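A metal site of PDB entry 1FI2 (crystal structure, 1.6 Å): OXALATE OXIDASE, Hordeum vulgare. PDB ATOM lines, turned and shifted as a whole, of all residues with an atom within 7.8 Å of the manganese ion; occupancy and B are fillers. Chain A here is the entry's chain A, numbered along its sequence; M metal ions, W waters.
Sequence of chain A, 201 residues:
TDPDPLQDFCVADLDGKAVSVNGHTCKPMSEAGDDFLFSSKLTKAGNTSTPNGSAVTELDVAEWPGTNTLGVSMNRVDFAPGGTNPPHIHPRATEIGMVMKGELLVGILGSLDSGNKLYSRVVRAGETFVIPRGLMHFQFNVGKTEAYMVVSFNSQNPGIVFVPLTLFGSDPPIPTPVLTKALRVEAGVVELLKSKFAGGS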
ATOM      1  N   ASN A  75     -16.754   6.896  13.876  1.00  0.00           N
ATOM      2  CA  ASN A  75     -17.765   5.942  13.408  1.00  0.00           C
ATOM      3  C   ASN A  75     -17.060   4.835  12.616  1.00  0.00           C
ATOM      4  O   ASN A  75     -15.921   4.996  12.207  1.00  0.00           O
ATOM      5  CB  ASN A  75     -18.886   6.583  12.640  1.00  0.00           C
ATOM      6  CG  ASN A  75     -18.724   7.039  11.221  1.00  0.00           C
ATOM      7  OD1 ASN A  75     -19.433   7.983  10.808  1.00  0.00           O
ATOM      8  ND2 ASN A  75     -17.861   6.432  10.416  1.00  0.00           N
ATOM      9  N   VAL A  77     -17.722   2.083   9.314  1.00  0.00           N
ATOM     10  CA  VAL A  77     -18.589   1.791   8.176  1.00  0.00           C
ATOM     11  C   VAL A  77     -18.168   0.455   7.556  1.00  0.00           C
ATOM     12  O   VAL A  77     -16.992   0.242   7.260  1.00  0.00           O
ATOM     13  CB  VAL A  77     -18.609   2.860   7.081  1.00  0.00           C
ATOM     14  CG1 VAL A  77     -19.692   2.556   6.049  1.00  0.00           C
ATOM     15  CG2 VAL A  77     -18.841   4.269   7.633  1.00  0.00           C
ATOM     16  N   ASN A  85     -21.153   3.917   0.552  1.00  0.00           N
ATOM     17  CA  ASN A  85     -21.556   5.000   1.465  1.00  0.00           C
ATOM     18  C   ASN A  85     -21.758   6.103   0.422  1.00  0.00           C
ATOM     19  O   ASN A  85     -20.780   6.520  -0.196  1.00  0.00           O
ATOM     20  CB  ASN A  85     -20.486   5.292   2.494  1.00  0.00           C
ATOM     21  CG  ASN A  85     -20.945   6.077   3.710  1.00  0.00           C
ATOM     22  OD1 ASN A  85     -22.138   6.260   3.927  1.00  0.00           O
ATOM     23  ND2 ASN A  85     -19.985   6.535   4.509  1.00  0.00           N
ATOM     24  N   PRO A  86     -23.006   6.413   0.083  1.00  0.00           N
ATOM     25  CA  PRO A  86     -23.334   7.319  -1.004  1.00  0.00           C
ATOM     26  C   PRO A  86     -22.811   8.722  -0.852  1.00  0.00           C
ATOM     27  O   PRO A  86     -22.428   9.120   0.232  1.00  0.00           O
ATOM     28  CB  PRO A  86     -24.858   7.278  -1.051  1.00  0.00           C
ATOM     29  CG  PRO A  86     -25.286   6.862   0.308  1.00  0.00           C
ATOM     30  CD  PRO A  86     -24.205   5.924   0.796  1.00  0.00           C
ATOM     31  N   HIS A  88     -22.207  12.059   0.314  1.00  0.00           N
ATOM     32  CA  HIS A  88     -22.760  12.724   1.487  1.00  0.00           C
ATOM     33  C   HIS A  88     -21.879  13.871   1.968  1.00  0.00           C
ATOM     34  O   HIS A  88     -20.795  14.107   1.425  1.00  0.00           O
ATOM     35  CB  HIS A  88     -22.981  11.712   2.621  1.00  0.00           C
ATOM     36  CG  HIS A  88     -21.719  11.096   3.136  1.00  0.00           C
ATOM     37  ND1 HIS A  88     -21.087  10.055   2.489  1.00  0.00           N
ATOM     38  CD2 HIS A  88     -20.970  11.387   4.230  1.00  0.00           C
ATOM     39  CE1 HIS A  88     -19.996   9.721   3.174  1.00  0.00           C
ATOM     40  NE2 HIS A  88     -19.910  10.510   4.224  1.00  0.00           N
ATOM     41  N   ILE A  89     -22.349  14.634   2.942  1.00  0.00           N
ATOM     42  CA  ILE A  89     -21.664  15.798   3.500  1.00  0.00           C
ATOM     43  C   ILE A  89     -21.805  15.832   5.024  1.00  0.00           C
ATOM     44  O   ILE A  89     -22.854  15.510   5.562  1.00  0.00           O
ATOM     45  CB  ILE A  89     -22.232  17.111   2.926  1.00  0.00           C
ATOM     46  CG1 ILE A  89     -21.757  17.341   1.493  1.00  0.00           C
ATOM     47  CG2 ILE A  89     -21.874  18.340   3.756  1.00  0.00           C
ATOM     48  CD1 ILE A  89     -22.756  17.940   0.552  1.00  0.00           C
ATOM     49  N   HIS A  90     -20.742  16.243   5.707  1.00  0.00           N
ATOM     50  CA  HIS A  90     -20.768  16.527   7.140  1.00  0.00           C
ATOM     51  C   HIS A  90     -20.744  18.043   7.303  1.00  0.00           C
ATOM     52  O   HIS A  90     -19.728  18.687   7.016  1.00  0.00           O
ATOM     53  CB  HIS A  90     -19.576  15.901   7.886  1.00  0.00           C
ATOM     54  CG  HIS A  90     -19.518  14.426   7.614  1.00  0.00           C
ATOM     55  ND1 HIS A  90     -20.442  13.552   8.130  1.00  0.00           N
ATOM     56  CD2 HIS A  90     -18.682  13.684   6.854  1.00  0.00           C
ATOM     57  CE1 HIS A  90     -20.185  12.331   7.708  1.00  0.00           C
ATOM     58  NE2 HIS A  90     -19.126  12.388   6.928  1.00  0.00           N
ATOM     59  N   ALA A  93     -17.879  19.328  10.318  1.00  0.00           N
ATOM     60  CA  ALA A  93     -16.579  18.737  10.603  1.00  0.00           C
ATOM     61  C   ALA A  93     -15.798  18.194   9.408  1.00  0.00           C
ATOM     62  O   ALA A  93     -16.334  17.768   8.403  1.00  0.00           O
ATOM     63  CB  ALA A  93     -16.774  17.554  11.563  1.00  0.00           C
ATOM     64  N   THR A  94     -14.493  18.106   9.640  1.00  0.00           N
ATOM     65  CA  THR A  94     -13.542  17.422   8.769  1.00  0.00           C
ATOM     66  C   THR A  94     -13.505  15.956   9.203  1.00  0.00           C
ATOM     67  O   THR A  94     -13.614  15.672  10.397  1.00  0.00           O
ATOM     68  CB  THR A  94     -12.126  18.016   8.903  1.00  0.00           C
ATOM     69  OG1 THR A  94     -12.092  19.366   8.431  1.00  0.00           O
ATOM     70  CG2 THR A  94     -11.099  17.208   8.107  1.00  0.00           C
ATOM     71  N   GLU A  95     -13.347  15.043   8.269  1.00  0.00           N
ATOM     72  CA  GLU A  95     -13.260  13.621   8.555  1.00  0.00           C
ATOM     73  C   GLU A  95     -11.876  13.105   8.188  1.00  0.00           C
ATOM     74  O   GLU A  95     -11.294  13.486   7.171  1.00  0.00           O
ATOM     75  CB  GLU A  95     -14.344  12.859   7.800  1.00  0.00           C
ATOM     76  CG  GLU A  95     -14.272  11.345   7.830  1.00  0.00           C
ATOM     77  CD  GLU A  95     -15.261  10.681   6.890  1.00  0.00           C
ATOM     78  OE1 GLU A  95     -16.133  11.395   6.346  1.00  0.00           O
ATOM     79  OE2 GLU A  95     -15.178   9.460   6.659  1.00  0.00           O
ATOM     80  N   ILE A  96     -11.351  12.220   9.040  1.00  0.00           N
ATOM     81  CA  ILE A  96     -10.043  11.607   8.802  1.00  0.00           C
ATOM     82  C   ILE A  96     -10.187  10.112   9.060  1.00  0.00           C
ATOM     83  O   ILE A  96     -10.635   9.712  10.132  1.00  0.00           O
ATOM     84  CB  ILE A  96      -8.946  12.301   9.610  1.00  0.00           C
ATOM     85  CG1 ILE A  96      -7.556  11.811   9.213  1.00  0.00           C
ATOM     86  CG2 ILE A  96      -9.162  12.162  11.112  1.00  0.00           C
ATOM     87  CD1 ILE A  96      -6.440  12.703   9.720  1.00  0.00           C
ATOM     88  N   PHE A 129      -7.253   8.627   4.481  1.00  0.00           N
ATOM     89  CA  PHE A 129      -7.833   9.683   3.658  1.00  0.00           C
ATOM     90  C   PHE A 129      -8.356  10.825   4.531  1.00  0.00           C
ATOM     91  O   PHE A 129      -8.637  10.638   5.718  1.00  0.00           O
ATOM     92  CB  PHE A 129      -8.984   9.142   2.809  1.00  0.00           C
ATOM     93  CG  PHE A 129     -10.131   8.522   3.552  1.00  0.00           C
ATOM     94  CD1 PHE A 129     -11.174   9.290   4.030  1.00  0.00           C
ATOM     95  CD2 PHE A 129     -10.172   7.146   3.752  1.00  0.00           C
ATOM     96  CE1 PHE A 129     -12.226   8.707   4.706  1.00  0.00           C
ATOM     97  CE2 PHE A 129     -11.223   6.553   4.427  1.00  0.00           C
ATOM     98  CZ  PHE A 129     -12.255   7.342   4.909  1.00  0.00           C
ATOM     99  N   ILE A 131     -11.200  14.212   4.472  1.00  0.00           N
ATOM    100  CA  ILE A 131     -12.294  14.903   3.801  1.00  0.00           C
ATOM    101  C   ILE A 131     -12.514  16.279   4.435  1.00  0.00           C
ATOM    102  O   ILE A 131     -13.049  16.361   5.546  1.00  0.00           O
ATOM    103  CB  ILE A 131     -13.647  14.171   3.993  1.00  0.00           C
ATOM    104  CG1 ILE A 131     -13.565  12.661   3.830  1.00  0.00           C
ATOM    105  CG2 ILE A 131     -14.694  14.789   3.067  1.00  0.00           C
ATOM    106  CD1 ILE A 131     -13.370  12.132   2.428  1.00  0.00           C
ATOM    107  N   LEU A 135     -17.511  19.184   2.372  1.00  0.00           N
ATOM    108  CA  LEU A 135     -17.438  18.812   0.962  1.00  0.00           C
ATOM    109  C   LEU A 135     -18.134  17.483   0.697  1.00  0.00           C
ATOM    110  O   LEU A 135     -18.141  16.604   1.559  1.00  0.00           O
ATOM    111  CB  LEU A 135     -15.981  18.745   0.495  1.00  0.00           C
ATOM    112  CG  LEU A 135     -15.182  20.046   0.603  1.00  0.00           C
ATOM    113  CD1 LEU A 135     -13.758  19.850   0.081  1.00  0.00           C
ATOM    114  CD2 LEU A 135     -15.858  21.179  -0.162  1.00  0.00           C
ATOM    115  N   MET A 136     -18.686  17.333  -0.496  1.00  0.00           N
ATOM    116  CA  MET A 136     -19.338  16.072  -0.875  1.00  0.00           C
ATOM    117  C   MET A 136     -18.302  14.976  -1.067  1.00  0.00           C
ATOM    118  O   MET A 136     -17.213  15.222  -1.602  1.00  0.00           O
ATOM    119  CB  MET A 136     -20.194  16.276  -2.138  1.00  0.00           C
ATOM    120  CG  MET A 136     -21.170  15.146  -2.392  1.00  0.00           C
ATOM    121  SD  MET A 136     -22.100  15.294  -3.936  1.00  0.00           S
ATOM    122  CE  MET A 136     -22.873  16.889  -3.716  1.00  0.00           C
ATOM    123  N   HIS A 137     -18.611  13.760  -0.617  1.00  0.00           N
ATOM    124  CA  HIS A 137     -17.684  12.635  -0.742  1.00  0.00           C
ATOM    125  C   HIS A 137     -18.423  11.305  -0.679  1.00  0.00           C
ATOM    126  O   HIS A 137     -19.593  11.266  -0.292  1.00  0.00           O
ATOM    127  CB  HIS A 137     -16.602  12.715   0.335  1.00  0.00           C
ATOM    128  CG  HIS A 137     -17.111  12.690   1.738  1.00  0.00           C
ATOM    129  ND1 HIS A 137     -17.841  13.735   2.272  1.00  0.00           N
ATOM    130  CD2 HIS A 137     -16.999  11.784   2.747  1.00  0.00           C
ATOM    131  CE1 HIS A 137     -18.158  13.470   3.514  1.00  0.00           C
ATOM    132  NE2 HIS A 137     -17.673  12.288   3.848  1.00  0.00           N
ATOM    133  N   PHE A 138     -17.765  10.224  -1.072  1.00  0.00           N
ATOM    134  CA  PHE A 138     -18.392   8.900  -1.065  1.00  0.00           C
ATOM    135  C   PHE A 138     -17.336   7.804  -0.996  1.00  0.00           C
ATOM    136  O   PHE A 138     -16.146   8.068  -1.183  1.00  0.00           O
ATOM    137  CB  PHE A 138     -19.186   8.700  -2.369  1.00  0.00           C
ATOM    138  CG  PHE A 138     -18.345   8.722  -3.622  1.00  0.00           C
ATOM    139  CD1 PHE A 138     -17.729   7.575  -4.088  1.00  0.00           C
ATOM    140  CD2 PHE A 138     -18.179   9.898  -4.333  1.00  0.00           C
ATOM    141  CE1 PHE A 138     -16.962   7.598  -5.238  1.00  0.00           C
ATOM    142  CE2 PHE A 138     -17.413   9.931  -5.482  1.00  0.00           C
ATOM    143  CZ  PHE A 138     -16.803   8.772  -5.942  1.00  0.00           C
ATOM    144  N   GLN A 139     -17.778   6.579  -0.737  1.00  0.00           N
ATOM    145  CA  GLN A 139     -16.909   5.409  -0.708  1.00  0.00           C
ATOM    146  C   GLN A 139     -17.640   4.279  -1.450  1.00  0.00           C
ATOM    147  O   GLN A 139     -18.868   4.165  -1.332  1.00  0.00           O
ATOM    148  CB  GLN A 139     -16.479   4.913   0.662  1.00  0.00           C
ATOM    149  CG  GLN A 139     -15.508   5.809   1.427  1.00  0.00           C
ATOM    150  CD  GLN A 139     -16.240   6.819   2.278  1.00  0.00           C
ATOM    151  OE1 GLN A 139     -17.336   6.548   2.779  1.00  0.00           O
ATOM    152  NE2 GLN A 139     -15.674   8.010   2.452  1.00  0.00           N
ATOM    153  N   MET A 149     -13.958   0.436   7.344  1.00  0.00           N
ATOM    154  CA  MET A 149     -13.106   1.568   7.705  1.00  0.00           C
ATOM    155  C   MET A 149     -13.576   2.158   9.029  1.00  0.00           C
ATOM    156  O   MET A 149     -14.718   1.966   9.440  1.00  0.00           O
ATOM    157  CB  MET A 149     -13.167   2.657   6.632  1.00  0.00           C
ATOM    158  CG  MET A 149     -14.555   3.213   6.408  1.00  0.00           C
ATOM    159  SD  MET A 149     -14.649   4.468   5.119  1.00  0.00           S
ATOM    160  CE  MET A 149     -16.268   5.189   5.457  1.00  0.00           C
ATOM    161  N   VAL A 151     -13.366   5.943  10.986  1.00  0.00           N
ATOM    162  CA  VAL A 151     -13.011   7.340  10.781  1.00  0.00           C
ATOM    163  C   VAL A 151     -13.208   8.156  12.062  1.00  0.00           C
ATOM    164  O   VAL A 151     -13.975   7.798  12.949  1.00  0.00           O
ATOM    165  CB  VAL A 151     -13.814   7.993   9.646  1.00  0.00           C
ATOM    166  CG1 VAL A 151     -13.802   7.167   8.366  1.00  0.00           C
ATOM    167  CG2 VAL A 151     -15.248   8.277  10.061  1.00  0.00           C
ATOM    168  N   PHE A 153     -13.713  12.401  13.489  1.00  0.00           N
ATOM    169  CA  PHE A 153     -14.190  13.719  13.087  1.00  0.00           C
ATOM    170  C   PHE A 153     -13.714  14.749  14.111  1.00  0.00           C
ATOM    171  O   PHE A 153     -13.522  14.433  15.283  1.00  0.00           O
ATOM    172  CB  PHE A 153     -15.713  13.812  13.043  1.00  0.00           C
ATOM    173  CG  PHE A 153     -16.386  12.850  12.098  1.00  0.00           C
ATOM    174  CD1 PHE A 153     -16.783  11.600  12.543  1.00  0.00           C
ATOM    175  CD2 PHE A 153     -16.620  13.204  10.779  1.00  0.00           C
ATOM    176  CE1 PHE A 153     -17.394  10.706  11.679  1.00  0.00           C
ATOM    177  CE2 PHE A 153     -17.231  12.310   9.915  1.00  0.00           C
ATOM    178  CZ  PHE A 153     -17.616  11.072  10.363  1.00  0.00           C
ATOM    179  N   GLY A 159     -22.803  15.530  11.992  1.00  0.00           N
ATOM    180  CA  GLY A 159     -24.030  15.570  11.216  1.00  0.00           C
ATOM    181  C   GLY A 159     -23.807  14.848   9.889  1.00  0.00           C
ATOM    182  O   GLY A 159     -22.658  14.702   9.474  1.00  0.00           O
ATOM    183  N   ILE A 160     -24.885  14.348   9.283  1.00  0.00           N
ATOM    184  CA  ILE A 160     -24.693  13.744   7.960  1.00  0.00           C
ATOM    185  C   ILE A 160     -25.856  14.116   7.047  1.00  0.00           C
ATOM    186  O   ILE A 160     -27.027  13.974   7.379  1.00  0.00           O
ATOM    187  CB  ILE A 160     -24.457  12.235   7.995  1.00  0.00           C
ATOM    188  CG1 ILE A 160     -24.245  11.704   6.565  1.00  0.00           C
ATOM    189  CG2 ILE A 160     -25.607  11.495   8.659  1.00  0.00           C
ATOM    190  CD1 ILE A 160     -23.563  10.355   6.499  1.00  0.00           C
ATOM    191  N   PHE A 162     -27.094  13.007   3.691  1.00  0.00           N
ATOM    192  CA  PHE A 162     -27.026  12.010   2.621  1.00  0.00           C
ATOM    193  C   PHE A 162     -27.652  12.649   1.372  1.00  0.00           C
ATOM    194  O   PHE A 162     -28.827  13.008   1.421  1.00  0.00           O
ATOM    195  CB  PHE A 162     -27.773  10.737   2.996  1.00  0.00           C
ATOM    196  CG  PHE A 162     -27.016   9.773   3.870  1.00  0.00           C
ATOM    197  CD1 PHE A 162     -27.442   9.533   5.167  1.00  0.00           C
ATOM    198  CD2 PHE A 162     -25.909   9.108   3.393  1.00  0.00           C
ATOM    199  CE1 PHE A 162     -26.767   8.630   5.967  1.00  0.00           C
ATOM    200  CE2 PHE A 162     -25.221   8.216   4.196  1.00  0.00           C
ATOM    201  CZ  PHE A 162     -25.654   7.976   5.486  1.00  0.00           C
HETATM  202 MN    MN M   1     -18.087  10.884   5.531  1.00  0.00          MN
HETATM  203  O   HOH W   1     -16.950   9.161   4.663  1.00  0.00           O
HETATM  204  O   HOH W   2     -19.093   9.383   7.167  1.00  0.00           O
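O of Glu 95 sits at hydrogen-bond distance from N of Ile 131 (2.8 Å).
A ring nitrogen (ND1) of His 137 sits at hydrogen-bond distance from the backbone carbonyl oxygen of Leu 135 (3.0 Å).
The backbone carbonyl oxygen of Pro 86 lies within hydrogen-bond range of a ring nitrogen (ND1) of His 88, 2.8 Å away.
O of Gly 159 lies within hydrogen-bond range of ND1 of His 90 (2.8 Å).
Four residues have an atom within 4 Å of the manganese ion: His 88, His 90, Glu 95 and His 137.
Along chain A the residues within 4 Å of the manganese ion span positions 88 to 137.
The nearest printed residue that does not touch the manganese ion is Phe 153 (4.7 Å).
The side-chain carboxylate (OE1) of Glu 95 binds the manganese ion (2.2 Å).
NE2 of His 137 is bound to the manganese ion, at 2.2 Å.
The manganese ion is bound by water W1 (2.2 Å).
The manganese ion is bound by NE2 of His 88 (2.3 Å).
NE2 of His 90 binds the manganese ion, at 2.3 Å.
Water W2 binds the manganese ion.
Water W1 lies within hydrogen-bond range of OE2 of Glu 95 and NE2 of Gln 139.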
